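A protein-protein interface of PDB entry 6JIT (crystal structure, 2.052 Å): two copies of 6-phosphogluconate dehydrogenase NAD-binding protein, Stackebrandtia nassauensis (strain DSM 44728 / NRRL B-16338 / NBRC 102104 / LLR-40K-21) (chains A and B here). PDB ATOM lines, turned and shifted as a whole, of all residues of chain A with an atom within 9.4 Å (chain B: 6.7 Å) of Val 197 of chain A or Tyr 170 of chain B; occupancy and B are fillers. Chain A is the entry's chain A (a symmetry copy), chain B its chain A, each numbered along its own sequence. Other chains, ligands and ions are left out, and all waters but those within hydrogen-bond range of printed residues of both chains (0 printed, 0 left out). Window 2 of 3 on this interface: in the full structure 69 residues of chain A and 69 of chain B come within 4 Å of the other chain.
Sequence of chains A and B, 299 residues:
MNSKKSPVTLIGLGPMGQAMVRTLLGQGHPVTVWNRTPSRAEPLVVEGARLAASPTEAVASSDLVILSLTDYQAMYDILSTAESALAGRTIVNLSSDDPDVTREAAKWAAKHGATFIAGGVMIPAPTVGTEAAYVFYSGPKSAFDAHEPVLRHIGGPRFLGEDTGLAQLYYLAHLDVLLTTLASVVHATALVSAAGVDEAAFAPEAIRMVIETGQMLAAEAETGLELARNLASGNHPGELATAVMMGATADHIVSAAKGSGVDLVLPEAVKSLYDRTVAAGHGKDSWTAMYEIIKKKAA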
ATOM      1  N   ALA A 188      16.456  -1.546 -16.658  1.00  0.00           N
ATOM      2  CA  ALA A 188      15.191  -1.051 -16.125  1.00  0.00           C
ATOM      3  C   ALA A 188      14.019  -1.475 -17.003  1.00  0.00           C
ATOM      4  O   ALA A 188      12.938  -1.797 -16.496  1.00  0.00           O
ATOM      5  CB  ALA A 188      15.229   0.470 -15.984  1.00  0.00           C
ATOM      6  N   THR A 189      14.216  -1.482 -18.325  1.00  0.00           N
ATOM      7  CA  THR A 189      13.152  -1.911 -19.226  1.00  0.00           C
ATOM      8  C   THR A 189      12.830  -3.391 -19.034  1.00  0.00           C
ATOM      9  O   THR A 189      11.655  -3.774 -19.006  1.00  0.00           O
ATOM     10  CB  THR A 189      13.540  -1.618 -20.679  1.00  0.00           C
ATOM     11  OG1 THR A 189      13.770  -0.211 -20.840  1.00  0.00           O
ATOM     12  CG2 THR A 189      12.430  -2.044 -21.626  1.00  0.00           C
ATOM     13  N   ALA A 190      13.854  -4.234 -18.887  1.00  0.00           N
ATOM     14  CA  ALA A 190      13.608  -5.651 -18.629  1.00  0.00           C
ATOM     15  C   ALA A 190      12.871  -5.850 -17.310  1.00  0.00           C
ATOM     16  O   ALA A 190      12.012  -6.734 -17.195  1.00  0.00           O
ATOM     17  CB  ALA A 190      14.924  -6.425 -18.622  1.00  0.00           C
ATOM     18  N   LEU A 191      13.199  -5.035 -16.307  1.00  0.00           N
ATOM     19  CA  LEU A 191      12.550  -5.147 -15.004  1.00  0.00           C
ATOM     20  C   LEU A 191      11.044  -4.932 -15.124  1.00  0.00           C
ATOM     21  O   LEU A 191      10.249  -5.702 -14.573  1.00  0.00           O
ATOM     22  CB  LEU A 191      13.175  -4.136 -14.041  1.00  0.00           C
ATOM     23  CG  LEU A 191      12.787  -4.170 -12.567  1.00  0.00           C
ATOM     24  CD1 LEU A 191      13.233  -5.475 -11.928  1.00  0.00           C
ATOM     25  CD2 LEU A 191      13.404  -2.976 -11.852  1.00  0.00           C
ATOM     26  N   VAL A 192      10.636  -3.896 -15.860  1.00  0.00           N
ATOM     27  CA  VAL A 192       9.215  -3.608 -16.031  1.00  0.00           C
ATOM     28  C   VAL A 192       8.570  -4.610 -16.984  1.00  0.00           C
ATOM     29  O   VAL A 192       7.455  -5.091 -16.740  1.00  0.00           O
ATOM     30  CB  VAL A 192       9.027  -2.160 -16.519  1.00  0.00           C
ATOM     31  CG1 VAL A 192       7.572  -1.893 -16.860  1.00  0.00           C
ATOM     32  CG2 VAL A 192       9.507  -1.188 -15.465  1.00  0.00           C
ATOM     33  N   SER A 193       9.251  -4.934 -18.085  1.00  0.00           N
ATOM     34  CA  SER A 193       8.680  -5.840 -19.074  1.00  0.00           C
ATOM     35  C   SER A 193       8.544  -7.261 -18.550  1.00  0.00           C
ATOM     36  O   SER A 193       7.776  -8.045 -19.118  1.00  0.00           O
ATOM     37  CB  SER A 193       9.524  -5.830 -20.348  1.00  0.00           C
ATOM     38  OG  SER A 193       9.353  -4.609 -21.051  1.00  0.00           O
ATOM     39  N   ALA A 194       9.266  -7.613 -17.483  1.00  0.00           N
ATOM     40  CA  ALA A 194       9.090  -8.926 -16.877  1.00  0.00           C
ATOM     41  C   ALA A 194       7.668  -9.137 -16.376  1.00  0.00           C
ATOM     42  O   ALA A 194       7.226 -10.284 -16.257  1.00  0.00           O
ATOM     43  CB  ALA A 194      10.085  -9.118 -15.730  1.00  0.00           C
ATOM     44  N   ALA A 195       6.943  -8.060 -16.088  1.00  0.00           N
ATOM     45  CA  ALA A 195       5.564  -8.145 -15.626  1.00  0.00           C
ATOM     46  C   ALA A 195       4.558  -8.207 -16.768  1.00  0.00           C
ATOM     47  O   ALA A 195       3.352  -8.221 -16.506  1.00  0.00           O
ATOM     48  CB  ALA A 195       5.236  -6.952 -14.721  1.00  0.00           C
ATOM     49  N   GLY A 196       5.020  -8.250 -18.016  1.00  0.00           N
ATOM     50  CA  GLY A 196       4.139  -8.248 -19.164  1.00  0.00           C
ATOM     51  C   GLY A 196       3.947  -6.900 -19.819  1.00  0.00           C
ATOM     52  O   GLY A 196       3.223  -6.815 -20.819  1.00  0.00           O
ATOM     53  N   VAL A 197       4.565  -5.844 -19.286  1.00  0.00           N
ATOM     54  CA  VAL A 197       4.466  -4.523 -19.896  1.00  0.00           C
ATOM     55  C   VAL A 197       5.209  -4.515 -21.225  1.00  0.00           C
ATOM     56  O   VAL A 197       6.302  -5.084 -21.352  1.00  0.00           O
ATOM     57  CB  VAL A 197       5.020  -3.451 -18.942  1.00  0.00           C
ATOM     58  CG1 VAL A 197       5.020  -2.080 -19.607  1.00  0.00           C
ATOM     59  CG2 VAL A 197       4.214  -3.422 -17.651  1.00  0.00           C
ATOM     60  N   ASP A 198       4.609  -3.876 -22.227  1.00  0.00           N
ATOM     61  CA  ASP A 198       5.249  -3.722 -23.529  1.00  0.00           C
ATOM     62  C   ASP A 198       6.531  -2.900 -23.402  1.00  0.00           C
ATOM     63  O   ASP A 198       6.527  -1.812 -22.821  1.00  0.00           O
ATOM     64  CB  ASP A 198       4.276  -3.051 -24.500  1.00  0.00           C
ATOM     65  CG  ASP A 198       4.861  -2.846 -25.892  1.00  0.00           C
ATOM     66  OD1 ASP A 198       5.905  -3.453 -26.217  1.00  0.00           O
ATOM     67  OD2 ASP A 198       4.265  -2.067 -26.668  1.00  0.00           O
ATOM     68  N   GLU A 199       7.631  -3.434 -23.947  1.00  0.00           N
ATOM     69  CA  GLU A 199       8.901  -2.709 -23.948  1.00  0.00           C
ATOM     70  C   GLU A 199       8.751  -1.311 -24.531  1.00  0.00           C
ATOM     71  O   GLU A 199       9.314  -0.344 -24.004  1.00  0.00           O
ATOM     72  CB  GLU A 199       9.962  -3.486 -24.735  1.00  0.00           C
ATOM     73  CG  GLU A 199      10.528  -4.705 -24.036  1.00  0.00           C
ATOM     74  CD  GLU A 199       9.682  -5.946 -24.234  1.00  0.00           C
ATOM     75  OE1 GLU A 199       8.585  -5.838 -24.822  1.00  0.00           O
ATOM     76  OE2 GLU A 199      10.122  -7.032 -23.802  1.00  0.00           O
ATOM     77  N   ALA A 200       7.988  -1.186 -25.622  1.00  0.00           N
ATOM     78  CA  ALA A 200       7.797   0.113 -26.256  1.00  0.00           C
ATOM     79  C   ALA A 200       7.093   1.108 -25.346  1.00  0.00           C
ATOM     80  O   ALA A 200       7.159   2.316 -25.600  1.00  0.00           O
ATOM     81  CB  ALA A 200       7.007  -0.045 -27.557  1.00  0.00           C
ATOM     82  N   ALA A 201       6.421   0.635 -24.294  1.00  0.00           N
ATOM     83  CA  ALA A 201       5.761   1.553 -23.374  1.00  0.00           C
ATOM     84  C   ALA A 201       6.734   2.127 -22.351  1.00  0.00           C
ATOM     85  O   ALA A 201       6.641   3.308 -22.002  1.00  0.00           O
ATOM     86  CB  ALA A 201       4.602   0.853 -22.665  1.00  0.00           C
ATOM     87  N   PHE A 202       7.662   1.319 -21.844  1.00  0.00           N
ATOM     88  CA  PHE A 202       8.514   1.794 -20.764  1.00  0.00           C
ATOM     89  C   PHE A 202       9.872   2.304 -21.226  1.00  0.00           C
ATOM     90  O   PHE A 202      10.406   3.227 -20.604  1.00  0.00           O
ATOM     91  CB  PHE A 202       8.731   0.703 -19.712  1.00  0.00           C
ATOM     92  CG  PHE A 202       9.421   1.204 -18.486  1.00  0.00           C
ATOM     93  CD1 PHE A 202       8.723   1.931 -17.535  1.00  0.00           C
ATOM     94  CD2 PHE A 202      10.777   0.996 -18.303  1.00  0.00           C
ATOM     95  CE1 PHE A 202       9.363   2.418 -16.410  1.00  0.00           C
ATOM     96  CE2 PHE A 202      11.420   1.482 -17.180  1.00  0.00           C
ATOM     97  CZ  PHE A 202      10.713   2.193 -16.235  1.00  0.00           C
ATOM     98  N   ALA A 203      10.442   1.728 -22.282  1.00  0.00           N
ATOM     99  CA  ALA A 203      11.737   2.192 -22.777  1.00  0.00           C
ATOM    100  C   ALA A 203      11.815   3.706 -22.963  1.00  0.00           C
ATOM    101  O   ALA A 203      12.840   4.288 -22.567  1.00  0.00           O
ATOM    102  CB  ALA A 203      12.084   1.466 -24.085  1.00  0.00           C
ATOM    103  N   PRO A 204      10.812   4.399 -23.520  1.00  0.00           N
ATOM    104  CA  PRO A 204      10.899   5.869 -23.562  1.00  0.00           C
ATOM    105  C   PRO A 204      10.918   6.513 -22.186  1.00  0.00           C
ATOM    106  O   PRO A 204      11.480   7.608 -22.036  1.00  0.00           O
ATOM    107  CB  PRO A 204       9.646   6.272 -24.354  1.00  0.00           C
ATOM    108  CG  PRO A 204       9.318   5.076 -25.169  1.00  0.00           C
ATOM    109  CD  PRO A 204       9.652   3.911 -24.288  1.00  0.00           C
ATOM    110  N   GLU A 205      10.316   5.875 -21.179  1.00  0.00           N
ATOM    111  CA  GLU A 205      10.360   6.422 -19.827  1.00  0.00           C
ATOM    112  C   GLU A 205      11.739   6.245 -19.206  1.00  0.00           C
ATOM    113  O   GLU A 205      12.244   7.150 -18.532  1.00  0.00           O
ATOM    114  CB  GLU A 205       9.290   5.765 -18.953  1.00  0.00           C
ATOM    115  CG  GLU A 205       7.870   6.155 -19.313  1.00  0.00           C
ATOM    116  CD  GLU A 205       7.698   7.658 -19.401  1.00  0.00           C
ATOM    117  OE1 GLU A 205       7.344   8.156 -20.492  1.00  0.00           O
ATOM    118  OE2 GLU A 205       7.936   8.342 -18.384  1.00  0.00           O
ATOM    119  N   ALA A 206      12.359   5.081 -19.410  1.00  0.00           N
ATOM    120  CA  ALA A 206      13.724   4.883 -18.937  1.00  0.00           C
ATOM    121  C   ALA A 206      14.676   5.873 -19.594  1.00  0.00           C
ATOM    122  O   ALA A 206      15.606   6.377 -18.954  1.00  0.00           O
ATOM    123  CB  ALA A 206      14.166   3.445 -19.207  1.00  0.00           C
ATOM    124  N   MET A 209      14.279   9.155 -17.960  1.00  0.00           N
ATOM    125  CA  MET A 209      14.929   9.174 -16.655  1.00  0.00           C
ATOM    126  C   MET A 209      16.399   9.566 -16.766  1.00  0.00           C
ATOM    127  O   MET A 209      16.937  10.197 -15.850  1.00  0.00           O
ATOM    128  CB  MET A 209      14.787   7.810 -15.979  1.00  0.00           C
ATOM    129  CG  MET A 209      15.119   7.830 -14.499  1.00  0.00           C
ATOM    130  SD  MET A 209      14.083   9.005 -13.602  1.00  0.00           S
ATOM    131  CE  MET A 209      15.009   9.158 -12.080  1.00  0.00           C
ATOM    132  N   ILE A 253      15.739  -2.713  -5.548  1.00  0.00           N
ATOM    133  CA  ILE A 253      15.930  -2.991  -6.969  1.00  0.00           C
ATOM    134  C   ILE A 253      16.448  -4.411  -7.166  1.00  0.00           C
ATOM    135  O   ILE A 253      16.006  -5.130  -8.071  1.00  0.00           O
ATOM    136  CB  ILE A 253      16.871  -1.945  -7.594  1.00  0.00           C
ATOM    137  CG1 ILE A 253      16.234  -0.553  -7.545  1.00  0.00           C
ATOM    138  CG2 ILE A 253      17.228  -2.325  -9.028  1.00  0.00           C
ATOM    139  CD1 ILE A 253      17.210   0.578  -7.816  1.00  0.00           C
ATOM    140  N   ALA A 256      13.582  -6.842  -6.360  1.00  0.00           N
ATOM    141  CA  ALA A 256      12.650  -6.795  -7.486  1.00  0.00           C
ATOM    142  C   ALA A 256      13.196  -7.564  -8.685  1.00  0.00           C
ATOM    143  O   ALA A 256      12.478  -8.354  -9.308  1.00  0.00           O
ATOM    144  CB  ALA A 256      12.358  -5.343  -7.865  1.00  0.00           C
ATOM    145  N   SER A 260      11.705 -10.848 -10.398  1.00  0.00           N
ATOM    146  CA  SER A 260      11.298 -10.770 -11.795  1.00  0.00           C
ATOM    147  C   SER A 260      12.013 -11.778 -12.684  1.00  0.00           C
ATOM    148  O   SER A 260      11.616 -11.945 -13.841  1.00  0.00           O
ATOM    149  CB  SER A 260      11.552  -9.362 -12.343  1.00  0.00           C
ATOM    150  OG  SER A 260      10.590  -8.432 -11.873  1.00  0.00           O
ATOM    151  N   PRO B  99       8.278  -4.853  -4.940  1.00  0.00           N
ATOM    152  CA  PRO B  99       6.918  -4.958  -5.501  1.00  0.00           C
ATOM    153  C   PRO B  99       6.110  -6.115  -4.940  1.00  0.00           C
ATOM    154  O   PRO B  99       4.907  -5.960  -4.704  1.00  0.00           O
ATOM    155  CB  PRO B  99       7.173  -5.118  -7.007  1.00  0.00           C
ATOM    156  CG  PRO B  99       8.511  -4.476  -7.228  1.00  0.00           C
ATOM    157  CD  PRO B  99       9.308  -4.797  -5.993  1.00  0.00           C
ATOM    158  N   MET B 122       7.713  10.469  -7.625  1.00  0.00           N
ATOM    159  CA  MET B 122       8.893  10.965  -8.319  1.00  0.00           C
ATOM    160  C   MET B 122       8.980  12.472  -8.111  1.00  0.00           C
ATOM    161  O   MET B 122       8.035  13.202  -8.427  1.00  0.00           O
ATOM    162  CB  MET B 122       8.831  10.622  -9.809  1.00  0.00           C
ATOM    163  CG  MET B 122       8.737   9.130 -10.110  1.00  0.00           C
ATOM    164  SD  MET B 122      10.305   8.262  -9.900  1.00  0.00           S
ATOM    165  CE  MET B 122      11.319   9.107 -11.111  1.00  0.00           C
ATOM    166  N   PHE B 136       3.218   7.533  -9.547  1.00  0.00           N
ATOM    167  CA  PHE B 136       2.638   6.310 -10.088  1.00  0.00           C
ATOM    168  C   PHE B 136       1.606   5.751  -9.114  1.00  0.00           C
ATOM    169  O   PHE B 136       1.815   5.756  -7.899  1.00  0.00           O
ATOM    170  CB  PHE B 136       3.724   5.261 -10.337  1.00  0.00           C
ATOM    171  CG  PHE B 136       4.842   5.728 -11.225  1.00  0.00           C
ATOM    172  CD1 PHE B 136       4.586   6.175 -12.512  1.00  0.00           C
ATOM    173  CD2 PHE B 136       6.157   5.690 -10.782  1.00  0.00           C
ATOM    174  CE1 PHE B 136       5.619   6.594 -13.337  1.00  0.00           C
ATOM    175  CE2 PHE B 136       7.198   6.107 -11.602  1.00  0.00           C
ATOM    176  CZ  PHE B 136       6.927   6.560 -12.881  1.00  0.00           C
ATOM    177  N   ARG B 158      -0.387   9.186 -12.280  1.00  0.00           N
ATOM    178  CA  ARG B 158      -0.282   8.300 -13.438  1.00  0.00           C
ATOM    179  C   ARG B 158      -0.744   6.909 -13.013  1.00  0.00           C
ATOM    180  O   ARG B 158       0.004   6.163 -12.372  1.00  0.00           O
ATOM    181  CB  ARG B 158       1.137   8.275 -14.005  1.00  0.00           C
ATOM    182  CG  ARG B 158       1.371   7.146 -15.005  1.00  0.00           C
ATOM    183  CD  ARG B 158       2.471   7.451 -16.014  1.00  0.00           C
ATOM    184  NE  ARG B 158       1.942   8.079 -17.221  1.00  0.00           N
ATOM    185  CZ  ARG B 158       2.498   7.976 -18.424  1.00  0.00           C
ATOM    186  NH1 ARG B 158       1.947   8.580 -19.466  1.00  0.00           N
ATOM    187  NH2 ARG B 158       3.602   7.259 -18.587  1.00  0.00           N
ATOM    188  N   LEU B 160      -1.270   3.170 -13.542  1.00  0.00           N
ATOM    189  CA  LEU B 160      -0.531   2.194 -14.334  1.00  0.00           C
ATOM    190  C   LEU B 160      -1.307   0.917 -14.612  1.00  0.00           C
ATOM    191  O   LEU B 160      -1.044   0.257 -15.621  1.00  0.00           O
ATOM    192  CB  LEU B 160       0.777   1.820 -13.628  1.00  0.00           C
ATOM    193  CG  LEU B 160       1.757   2.965 -13.384  1.00  0.00           C
ATOM    194  CD1 LEU B 160       2.957   2.466 -12.606  1.00  0.00           C
ATOM    195  CD2 LEU B 160       2.185   3.582 -14.705  1.00  0.00           C
ATOM    196  N   GLY B 165       1.401  -4.161  -7.441  1.00  0.00           N
ATOM    197  CA  GLY B 165       2.853  -4.115  -7.504  1.00  0.00           C
ATOM    198  C   GLY B 165       3.429  -3.222  -8.590  1.00  0.00           C
ATOM    199  O   GLY B 165       4.645  -3.000  -8.590  1.00  0.00           O
ATOM    200  N   LEU B 166       2.598  -2.694  -9.493  1.00  0.00           N
ATOM    201  CA  LEU B 166       3.123  -1.942 -10.632  1.00  0.00           C
ATOM    202  C   LEU B 166       3.789  -0.637 -10.204  1.00  0.00           C
ATOM    203  O   LEU B 166       4.836  -0.267 -10.747  1.00  0.00           O
ATOM    204  CB  LEU B 166       2.009  -1.656 -11.639  1.00  0.00           C
ATOM    205  CG  LEU B 166       1.535  -2.834 -12.496  1.00  0.00           C
ATOM    206  CD1 LEU B 166       0.323  -2.434 -13.314  1.00  0.00           C
ATOM    207  CD2 LEU B 166       2.655  -3.319 -13.404  1.00  0.00           C
ATOM    208  N   ALA B 167       3.193   0.082  -9.247  1.00  0.00           N
ATOM    209  CA  ALA B 167       3.697   1.410  -8.900  1.00  0.00           C
ATOM    210  C   ALA B 167       5.136   1.351  -8.402  1.00  0.00           C
ATOM    211  O   ALA B 167       5.971   2.172  -8.798  1.00  0.00           O
ATOM    212  CB  ALA B 167       2.796   2.065  -7.853  1.00  0.00           C
ATOM    213  N   GLN B 168       5.449   0.384  -7.540  1.00  0.00           N
ATOM    214  CA  GLN B 168       6.817   0.282  -7.051  1.00  0.00           C
ATOM    215  C   GLN B 168       7.740  -0.370  -8.071  1.00  0.00           C
ATOM    216  O   GLN B 168       8.942  -0.086  -8.075  1.00  0.00           O
ATOM    217  CB  GLN B 168       6.853  -0.475  -5.723  1.00  0.00           C
ATOM    218  CG  GLN B 168       6.441   0.395  -4.537  1.00  0.00           C
ATOM    219  CD  GLN B 168       7.301   1.641  -4.416  1.00  0.00           C
ATOM    220  OE1 GLN B 168       8.530   1.560  -4.425  1.00  0.00           O
ATOM    221  NE2 GLN B 168       6.659   2.802  -4.322  1.00  0.00           N
ATOM    222  N   LEU B 169       7.208  -1.227  -8.944  1.00  0.00           N
ATOM    223  CA  LEU B 169       8.021  -1.760 -10.035  1.00  0.00           C
ATOM    224  C   LEU B 169       8.497  -0.641 -10.957  1.00  0.00           C
ATOM    225  O   LEU B 169       9.686  -0.557 -11.286  1.00  0.00           O
ATOM    226  CB  LEU B 169       7.230  -2.807 -10.819  1.00  0.00           C
ATOM    227  CG  LEU B 169       7.950  -3.404 -12.031  1.00  0.00           C
ATOM    228  CD1 LEU B 169       9.212  -4.135 -11.603  1.00  0.00           C
ATOM    229  CD2 LEU B 169       7.020  -4.336 -12.793  1.00  0.00           C
ATOM    230  N   TYR B 170       7.577   0.231 -11.384  1.00  0.00           N
ATOM    231  CA  TYR B 170       7.957   1.370 -12.217  1.00  0.00           C
ATOM    232  C   TYR B 170       8.880   2.321 -11.464  1.00  0.00           C
ATOM    233  O   TYR B 170       9.859   2.827 -12.029  1.00  0.00           O
ATOM    234  CB  TYR B 170       6.716   2.134 -12.675  1.00  0.00           C
ATOM    235  CG  TYR B 170       5.945   1.562 -13.846  1.00  0.00           C
ATOM    236  CD1 TYR B 170       5.392   0.286 -13.796  1.00  0.00           C
ATOM    237  CD2 TYR B 170       5.708   2.334 -14.980  1.00  0.00           C
ATOM    238  CE1 TYR B 170       4.655  -0.216 -14.862  1.00  0.00           C
ATOM    239  CE2 TYR B 170       4.981   1.839 -16.050  1.00  0.00           C
ATOM    240  CZ  TYR B 170       4.452   0.567 -15.983  1.00  0.00           C
ATOM    241  OH  TYR B 170       3.721   0.081 -17.049  1.00  0.00           O
ATOM    242  N   TYR B 171       8.560   2.599 -10.198  1.00  0.00           N
ATOM    243  CA  TYR B 171       9.388   3.491  -9.394  1.00  0.00           C
ATOM    244  C   TYR B 171      10.813   2.962  -9.282  1.00  0.00           C
ATOM    245  O   TYR B 171      11.779   3.693  -9.528  1.00  0.00           O
ATOM    246  CB  TYR B 171       8.768   3.674  -8.006  1.00  0.00           C
ATOM    247  CG  TYR B 171       9.630   4.475  -7.058  1.00  0.00           C
ATOM    248  CD1 TYR B 171       9.617   5.864  -7.084  1.00  0.00           C
ATOM    249  CD2 TYR B 171      10.462   3.844  -6.141  1.00  0.00           C
ATOM    250  CE1 TYR B 171      10.411   6.603  -6.220  1.00  0.00           C
ATOM    251  CE2 TYR B 171      11.259   4.573  -5.278  1.00  0.00           C
ATOM    252  CZ  TYR B 171      11.228   5.951  -5.321  1.00  0.00           C
ATOM    253  OH  TYR B 171      12.019   6.677  -4.463  1.00  0.00           O
ATOM    254  N   LEU B 172      10.961   1.684  -8.923  1.00  0.00           N
ATOM    255  CA  LEU B 172      12.289   1.106  -8.746  1.00  0.00           C
ATOM    256  C   LEU B 172      13.051   1.014 -10.064  1.00  0.00           C
ATOM    257  O   LEU B 172      14.282   1.121 -10.075  1.00  0.00           O
ATOM    258  CB  LEU B 172      12.177  -0.274  -8.091  1.00  0.00           C
ATOM    259  CG  LEU B 172      11.681  -0.296  -6.636  1.00  0.00           C
ATOM    260  CD1 LEU B 172      11.477  -1.725  -6.145  1.00  0.00           C
ATOM    261  CD2 LEU B 172      12.634   0.458  -5.720  1.00  0.00           C
ATOM    262  N   ALA B 173      12.344   0.818 -11.180  1.00  0.00           N
ATOM    263  CA  ALA B 173      13.008   0.811 -12.479  1.00  0.00           C
ATOM    264  C   ALA B 173      13.539   2.194 -12.832  1.00  0.00           C
ATOM    265  O   ALA B 173      14.639   2.320 -13.379  1.00  0.00           O
ATOM    266  CB  ALA B 173      12.051   0.312 -13.559  1.00  0.00           C
ATOM    267  N   HIS B 174      12.770   3.243 -12.529  1.00  0.00           N
ATOM    268  CA  HIS B 174      13.283   4.600 -12.686  1.00  0.00           C
ATOM    269  C   HIS B 174      14.509   4.826 -11.808  1.00  0.00           C
ATOM    270  O   HIS B 174      15.507   5.402 -12.258  1.00  0.00           O
ATOM    271  CB  HIS B 174      12.197   5.624 -12.348  1.00  0.00           C
ATOM    272  CG  HIS B 174      11.218   5.867 -13.455  1.00  0.00           C
ATOM    273  ND1 HIS B 174      10.260   4.947 -13.820  1.00  0.00           N
ATOM    274  CD2 HIS B 174      11.042   6.936 -14.268  1.00  0.00           C
ATOM    275  CE1 HIS B 174       9.541   5.434 -14.816  1.00  0.00           C
ATOM    276  NE2 HIS B 174       9.995   6.640 -15.107  1.00  0.00           N
ATOM    277  N   LEU B 175      14.448   4.375 -10.549  1.00  0.00           N
ATOM    278  CA  LEU B 175      15.581   4.528  -9.640  1.00  0.00           C
ATOM    279  C   LEU B 175      16.743   3.630 -10.040  1.00  0.00           C
ATOM    280  O   LEU B 175      17.900   3.933  -9.724  1.00  0.00           O
ATOM    281  CB  LEU B 175      15.149   4.230  -8.202  1.00  0.00           C
ATOM    282  CG  LEU B 175      14.661   5.402  -7.343  1.00  0.00           C
ATOM    283  CD1 LEU B 175      15.823   6.328  -6.991  1.00  0.00           C
ATOM    284  CD2 LEU B 175      13.561   6.178  -8.040  1.00  0.00           C
ATOM    285  N   TYR B 291      19.817  -7.046 -23.959  1.00  0.00           N
ATOM    286  CA  TYR B 291      18.483  -7.265 -23.407  1.00  0.00           C
ATOM    287  C   TYR B 291      18.126  -8.747 -23.384  1.00  0.00           C
ATOM    288  O   TYR B 291      17.451  -9.215 -22.460  1.00  0.00           O
ATOM    289  CB  TYR B 291      17.454  -6.478 -24.219  1.00  0.00           C
ATOM    290  CG  TYR B 291      16.041  -6.591 -23.694  1.00  0.00           C
ATOM    291  CD1 TYR B 291      15.656  -5.926 -22.534  1.00  0.00           C
ATOM    292  CD2 TYR B 291      15.089  -7.355 -24.360  1.00  0.00           C
ATOM    293  CE1 TYR B 291      14.366  -6.025 -22.050  1.00  0.00           C
ATOM    294  CE2 TYR B 291      13.795  -7.460 -23.882  1.00  0.00           C
ATOM    295  CZ  TYR B 291      13.440  -6.792 -22.728  1.00  0.00           C
ATOM    296  OH  TYR B 291      12.158  -6.888 -22.241  1.00  0.00           O
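The side-chain hydroxyl (OH) of Tyr 291 of chain B lies within hydrogen-bond range of the side-chain carboxylate (OE2) of Glu 199 of chain A, 2.6 Å away.
O of Ala 256 of chain A sits at hydrogen-bond distance from OG of Ser 260 of chain A.
OG of Ser 193 of chain A sits at hydrogen-bond distance from O of Thr 189 of chain A, 3.2 Å away.
The backbone carbonyl oxygen (O) of Tyr 170 of chain B sits at hydrogen-bond distance from a ring nitrogen (ND1) of His 174 of chain B (2.8 Å).
OG of Ser 193 of chain A sits at hydrogen-bond distance from O of Val 197 of chain A (3.1 Å).
Ala 173 of chain B touches Leu 191 of chain A (CA to CD2, 3.9 Å).
Val 192 of chain A touches Leu 169 of chain B.
Tyr 170 of chain B touches Val 192 of chain A (CE1 to CG1, 3.9 Å).
CB of Ala 173 of chain B touches CG2 of Val 192 of chain A (3.5 Å).
Ser 193 of chain A touches Tyr 291 of chain B (CB to OH, 3.4 Å).
Ala 195 of chain A touches Leu 169 of chain B (CB to CD2, 3.7 Å).
Phe 202 of chain A touches His 174 of chain B (CE1 to CE1, 3.4 Å).
Met 209 of chain A touches Met 122 of chain B.
Ile 253 of chain A touches Leu 172 of chain B.
CD1 of Ile 253 of chain A touches C of Leu 175 of chain B, at 3.8 Å.
Of chain B, only Tyr 170 (3.6 Å) comes within 4 Å of Val 197 of chain A.
Of the printed residues of chain A, Pro 99 of chain B touches Ala 256.
Of the printed residues of chain B, Ile 253 of chain A touches Leu 172 and Leu 175.
Of the printed residues of chain A, Leu 172 of chain B touches Ile 253 (3.6 Å).
Ala 200 of chain A touches none of the printed residues of chain B.
Thr 189 of chain A touches none of the printed residues of chain B.
The nearest residue of chain A that does not touch Tyr 170 of chain B is Ala 201 of chain A (5.7 Å).
The nearest printed residue of chain B that does not touch Met 209 of chain A is Leu 175 of chain B (5.1 Å).
Hydrophobic or aromatic side chains of chain A within 4 Å of the printed part of chain B: Ala 188, Ala 190, Leu 191, Val 192, Ala 195, Val 197, Phe 202, Met 209, Ile 253 and Ala 256.
Of the 17 printed residues of chain B, 9 touch a printed residue of chain A.
Printed residues of chain B that touch a printed residue of chain A: Pro 99, Met 122, Leu 169, Tyr 170, Leu 172, Ala 173, His 174, Leu 175 and Tyr 291.
Among the printed residues, no Asp or Glu carboxylate lies within 4 Å of a Lys or Arg side-chain nitrogen of the other chain.
No position is printed for both chains.
Of the 19 pairs that touch across the chains among the printed residues, none has its exchanged pair printed and touching as well.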
